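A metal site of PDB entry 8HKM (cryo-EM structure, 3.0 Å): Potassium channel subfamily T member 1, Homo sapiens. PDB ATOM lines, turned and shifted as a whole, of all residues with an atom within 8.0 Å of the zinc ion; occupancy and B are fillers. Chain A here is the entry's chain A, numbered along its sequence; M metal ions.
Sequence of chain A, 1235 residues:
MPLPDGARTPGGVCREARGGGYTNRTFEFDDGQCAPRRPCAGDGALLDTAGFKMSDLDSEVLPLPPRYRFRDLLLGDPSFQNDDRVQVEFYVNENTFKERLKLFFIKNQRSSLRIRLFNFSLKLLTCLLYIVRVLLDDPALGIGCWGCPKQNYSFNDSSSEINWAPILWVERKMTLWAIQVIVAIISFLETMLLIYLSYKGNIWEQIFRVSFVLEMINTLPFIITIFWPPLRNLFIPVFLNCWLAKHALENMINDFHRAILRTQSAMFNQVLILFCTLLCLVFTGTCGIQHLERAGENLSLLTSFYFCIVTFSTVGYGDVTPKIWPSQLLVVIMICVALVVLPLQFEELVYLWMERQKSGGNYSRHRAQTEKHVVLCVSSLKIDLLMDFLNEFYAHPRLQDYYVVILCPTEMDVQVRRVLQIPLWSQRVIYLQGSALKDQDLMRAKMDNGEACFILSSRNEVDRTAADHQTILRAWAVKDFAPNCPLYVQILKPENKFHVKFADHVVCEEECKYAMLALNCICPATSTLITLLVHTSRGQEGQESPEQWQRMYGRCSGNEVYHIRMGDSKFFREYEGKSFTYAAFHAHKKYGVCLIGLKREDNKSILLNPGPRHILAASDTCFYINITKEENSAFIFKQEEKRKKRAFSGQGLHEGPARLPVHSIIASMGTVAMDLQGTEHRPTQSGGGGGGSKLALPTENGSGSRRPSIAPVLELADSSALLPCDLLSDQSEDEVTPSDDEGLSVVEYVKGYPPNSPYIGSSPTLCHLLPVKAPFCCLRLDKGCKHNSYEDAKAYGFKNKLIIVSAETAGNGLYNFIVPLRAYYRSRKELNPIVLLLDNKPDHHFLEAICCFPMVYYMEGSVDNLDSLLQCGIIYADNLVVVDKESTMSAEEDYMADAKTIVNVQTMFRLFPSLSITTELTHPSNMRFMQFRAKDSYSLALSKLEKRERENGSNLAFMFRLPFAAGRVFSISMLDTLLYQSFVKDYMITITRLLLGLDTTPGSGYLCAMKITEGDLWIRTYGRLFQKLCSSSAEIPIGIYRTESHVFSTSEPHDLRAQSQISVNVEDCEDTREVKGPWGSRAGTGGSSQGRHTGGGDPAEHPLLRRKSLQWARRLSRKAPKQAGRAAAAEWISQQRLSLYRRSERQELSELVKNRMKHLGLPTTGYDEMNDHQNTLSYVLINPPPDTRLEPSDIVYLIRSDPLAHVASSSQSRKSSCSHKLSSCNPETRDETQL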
ATOM      1  N   ALA A 774      -6.392  23.595   5.685  1.00  0.00           N
ATOM      2  CA  ALA A 774      -7.609  23.290   4.942  1.00  0.00           C
ATOM      3  C   ALA A 774      -8.758  23.011   5.907  1.00  0.00           C
ATOM      4  O   ALA A 774      -8.567  22.271   6.874  1.00  0.00           O
ATOM      5  CB  ALA A 774      -7.392  22.081   4.028  1.00  0.00           C
ATOM      6  N   PRO A 775      -9.932  23.595   5.682  1.00  0.00           N
ATOM      7  CA  PRO A 775     -11.084  23.249   6.518  1.00  0.00           C
ATOM      8  C   PRO A 775     -11.485  21.792   6.330  1.00  0.00           C
ATOM      9  O   PRO A 775     -11.241  21.190   5.278  1.00  0.00           O
ATOM     10  CB  PRO A 775     -12.185  24.195   6.018  1.00  0.00           C
ATOM     11  CG  PRO A 775     -11.755  24.594   4.649  1.00  0.00           C
ATOM     12  CD  PRO A 775     -10.252  24.621   4.686  1.00  0.00           C
ATOM     13  N   PHE A 776     -12.100  21.233   7.366  1.00  0.00           N
ATOM     14  CA  PHE A 776     -12.479  19.829   7.343  1.00  0.00           C
ATOM     15  C   PHE A 776     -13.459  19.505   6.225  1.00  0.00           C
ATOM     16  O   PHE A 776     -13.580  18.341   5.824  1.00  0.00           O
ATOM     17  CB  PHE A 776     -13.082  19.412   8.686  1.00  0.00           C
ATOM     18  CG  PHE A 776     -12.099  19.453   9.837  1.00  0.00           C
ATOM     19  CD1 PHE A 776     -10.766  19.746   9.629  1.00  0.00           C
ATOM     20  CD2 PHE A 776     -12.527  19.195  11.127  1.00  0.00           C
ATOM     21  CE1 PHE A 776      -9.876  19.785  10.676  1.00  0.00           C
ATOM     22  CE2 PHE A 776     -11.638  19.237  12.184  1.00  0.00           C
ATOM     23  CZ  PHE A 776     -10.309  19.536  11.963  1.00  0.00           C
ATOM     24  N   CYS A 777     -14.175  20.512   5.711  1.00  0.00           N
ATOM     25  CA  CYS A 777     -15.077  20.277   4.590  1.00  0.00           C
ATOM     26  C   CYS A 777     -14.313  20.006   3.301  1.00  0.00           C
ATOM     27  O   CYS A 777     -14.721  19.150   2.504  1.00  0.00           O
ATOM     28  CB  CYS A 777     -16.010  21.479   4.415  1.00  0.00           C
ATOM     29  SG  CYS A 777     -15.162  23.022   3.986  1.00  0.00           S
ATOM     30  N   CYS A 778     -13.208  20.709   3.093  1.00  0.00           N
ATOM     31  CA  CYS A 778     -12.455  20.588   1.846  1.00  0.00           C
ATOM     32  C   CYS A 778     -11.666  19.281   1.751  1.00  0.00           C
ATOM     33  O   CYS A 778     -11.277  18.894   0.649  1.00  0.00           O
ATOM     34  CB  CYS A 778     -11.512  21.772   1.679  1.00  0.00           C
ATOM     35  SG  CYS A 778     -12.341  23.347   1.355  1.00  0.00           S
ATOM     36  N   LEU A 779     -11.417  18.611   2.873  1.00  0.00           N
ATOM     37  CA  LEU A 779     -10.677  17.358   2.883  1.00  0.00           C
ATOM     38  C   LEU A 779     -11.532  16.170   2.457  1.00  0.00           C
ATOM     39  O   LEU A 779     -11.055  15.034   2.532  1.00  0.00           O
ATOM     40  CB  LEU A 779     -10.094  17.098   4.277  1.00  0.00           C
ATOM     41  CG  LEU A 779      -9.142  18.153   4.822  1.00  0.00           C
ATOM     42  CD1 LEU A 779      -8.663  17.767   6.217  1.00  0.00           C
ATOM     43  CD2 LEU A 779      -7.962  18.353   3.892  1.00  0.00           C
ATOM     44  N   ARG A 780     -12.754  16.404   1.998  1.00  0.00           N
ATOM     45  CA  ARG A 780     -13.684  15.341   1.644  1.00  0.00           C
ATOM     46  C   ARG A 780     -13.908  15.322   0.146  1.00  0.00           C
ATOM     47  O   ARG A 780     -14.005  16.372  -0.497  1.00  0.00           O
ATOM     48  CB  ARG A 780     -15.021  15.533   2.369  1.00  0.00           C
ATOM     49  CG  ARG A 780     -16.100  14.555   1.945  1.00  0.00           C
ATOM     50  CD  ARG A 780     -16.339  13.499   3.011  1.00  0.00           C
ATOM     51  NE  ARG A 780     -16.942  14.062   4.209  1.00  0.00           N
ATOM     52  CZ  ARG A 780     -18.183  13.819   4.602  1.00  0.00           C
ATOM     53  NH1 ARG A 780     -18.990  13.038   3.897  1.00  0.00           N
ATOM     54  NH2 ARG A 780     -18.643  14.383   5.712  1.00  0.00           N
ATOM     55  N   LYS A 783     -18.417  14.630  -0.677  1.00  0.00           N
ATOM     56  CA  LYS A 783     -19.303  15.747  -0.355  1.00  0.00           C
ATOM     57  C   LYS A 783     -18.704  17.072  -0.827  1.00  0.00           C
ATOM     58  O   LYS A 783     -17.485  17.297  -0.729  1.00  0.00           O
ATOM     59  CB  LYS A 783     -19.559  15.795   1.154  1.00  0.00           C
ATOM     60  CG  LYS A 783     -20.099  17.124   1.667  1.00  0.00           C
ATOM     61  CD  LYS A 783     -20.288  17.111   3.168  1.00  0.00           C
ATOM     62  CE  LYS A 783     -19.407  18.155   3.833  1.00  0.00           C
ATOM     63  NZ  LYS A 783     -20.115  19.443   4.025  1.00  0.00           N
ATOM     64  N   GLY A 784     -19.568  17.954  -1.335  1.00  0.00           N
ATOM     65  CA  GLY A 784     -19.167  19.272  -1.755  1.00  0.00           C
ATOM     66  C   GLY A 784     -19.352  20.303  -0.644  1.00  0.00           C
ATOM     67  O   GLY A 784     -20.034  20.061   0.353  1.00  0.00           O
ATOM     68  N   CYS A 785     -18.738  21.465  -0.842  1.00  0.00           N
ATOM     69  CA  CYS A 785     -18.761  22.506   0.180  1.00  0.00           C
ATOM     70  C   CYS A 785     -18.879  23.897  -0.432  1.00  0.00           C
ATOM     71  O   CYS A 785     -19.177  24.035  -1.616  1.00  0.00           O
ATOM     72  CB  CYS A 785     -17.507  22.427   1.060  1.00  0.00           C
ATOM     73  SG  CYS A 785     -15.984  22.946   0.219  1.00  0.00           S
ATOM     74  N   LYS A 786     -18.646  24.935   0.380  1.00  0.00           N
ATOM     75  CA  LYS A 786     -18.691  26.299  -0.144  1.00  0.00           C
ATOM     76  C   LYS A 786     -17.521  26.563  -1.081  1.00  0.00           C
ATOM     77  O   LYS A 786     -17.703  27.196  -2.134  1.00  0.00           O
ATOM     78  CB  LYS A 786     -18.669  27.304   1.018  1.00  0.00           C
ATOM     79  CG  LYS A 786     -19.751  27.075   2.060  1.00  0.00           C
ATOM     80  CD  LYS A 786     -19.958  28.324   2.902  1.00  0.00           C
ATOM     81  CE  LYS A 786     -18.679  28.724   3.616  1.00  0.00           C
ATOM     82  NZ  LYS A 786     -18.838  29.988   4.387  1.00  0.00           N
ATOM     83  N   HIS A 787     -16.324  26.092  -0.728  1.00  0.00           N
ATOM     84  CA  HIS A 787     -15.155  26.340  -1.567  1.00  0.00           C
ATOM     85  C   HIS A 787     -15.211  25.564  -2.877  1.00  0.00           C
ATOM     86  O   HIS A 787     -14.751  26.052  -3.912  1.00  0.00           O
ATOM     87  CB  HIS A 787     -13.873  25.988  -0.809  1.00  0.00           C
ATOM     88  CG  HIS A 787     -13.865  26.454   0.608  1.00  0.00           C
ATOM     89  ND1 HIS A 787     -14.559  25.805   1.608  1.00  0.00           N
ATOM     90  CD2 HIS A 787     -13.234  27.495   1.204  1.00  0.00           C
ATOM     91  CE1 HIS A 787     -14.363  26.437   2.753  1.00  0.00           C
ATOM     92  NE2 HIS A 787     -13.553  27.464   2.540  1.00  0.00           N
ATOM     93  N   ASN A 788     -15.775  24.361  -2.850  1.00  0.00           N
ATOM     94  CA  ASN A 788     -15.838  23.518  -4.027  1.00  0.00           C
ATOM     95  C   ASN A 788     -17.076  22.632  -3.983  1.00  0.00           C
ATOM     96  O   ASN A 788     -17.532  22.244  -2.901  1.00  0.00           O
ATOM     97  CB  ASN A 788     -14.544  22.689  -4.172  1.00  0.00           C
ATOM     98  CG  ASN A 788     -14.329  21.697  -3.041  1.00  0.00           C
ATOM     99  OD1 ASN A 788     -15.281  21.130  -2.488  1.00  0.00           O
ATOM    100  ND2 ASN A 788     -13.071  21.476  -2.674  1.00  0.00           N
ATOM    101  N   SER A 789     -17.620  22.358  -5.158  1.00  0.00           N
ATOM    102  CA  SER A 789     -18.777  21.477  -5.304  1.00  0.00           C
ATOM    103  C   SER A 789     -18.426  20.175  -6.001  1.00  0.00           C
ATOM    104  O   SER A 789     -19.329  19.424  -6.382  1.00  0.00           O
ATOM    105  CB  SER A 789     -19.902  22.198  -6.060  1.00  0.00           C
ATOM    106  OG  SER A 789     -21.014  21.338  -6.248  1.00  0.00           O
ATOM    107  N   TYR A 796     -12.290  17.183  -9.741  1.00  0.00           N
ATOM    108  CA  TYR A 796     -11.128  17.900  -9.239  1.00  0.00           C
ATOM    109  C   TYR A 796     -10.118  18.201 -10.339  1.00  0.00           C
ATOM    110  O   TYR A 796      -9.401  19.204 -10.254  1.00  0.00           O
ATOM    111  CB  TYR A 796     -10.452  17.107  -8.109  1.00  0.00           C
ATOM    112  CG  TYR A 796     -11.076  17.311  -6.745  1.00  0.00           C
ATOM    113  CD1 TYR A 796     -12.301  16.734  -6.428  1.00  0.00           C
ATOM    114  CD2 TYR A 796     -10.453  18.088  -5.788  1.00  0.00           C
ATOM    115  CE1 TYR A 796     -12.868  16.931  -5.180  1.00  0.00           C
ATOM    116  CE2 TYR A 796     -11.011  18.289  -4.541  1.00  0.00           C
ATOM    117  CZ  TYR A 796     -12.228  17.696  -4.250  1.00  0.00           C
ATOM    118  OH  TYR A 796     -12.794  17.890  -3.012  1.00  0.00           O
HETATM  119 ZN    ZN M   1     -14.564  23.749   1.862  1.00  0.00          ZN
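Within 4 Å of the zinc ion: Cys 777, Cys 778, Cys 785 and His 787.
Along chain A the residues within 4 Å of the zinc ion span positions 777 to 787.
The nearest printed residue that does not touch the zinc ion is Pro 775 (4.05 Å).
The side-chain sulfur (SG) of Cys 785 lies close to the side-chain amide oxygen (OD1) of Asn 788 (3.3 Å).
The zinc ion is bound by a ring nitrogen (ND1) of His 787 (2.1 Å), the side-chain sulfur of Cys 778 (2.3 Å), the side-chain sulfur of Cys 785 (2.3 Å) and the side-chain sulfur of Cys 777 (2.3 Å).
The zinc ion has four donor atoms within binding distance.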
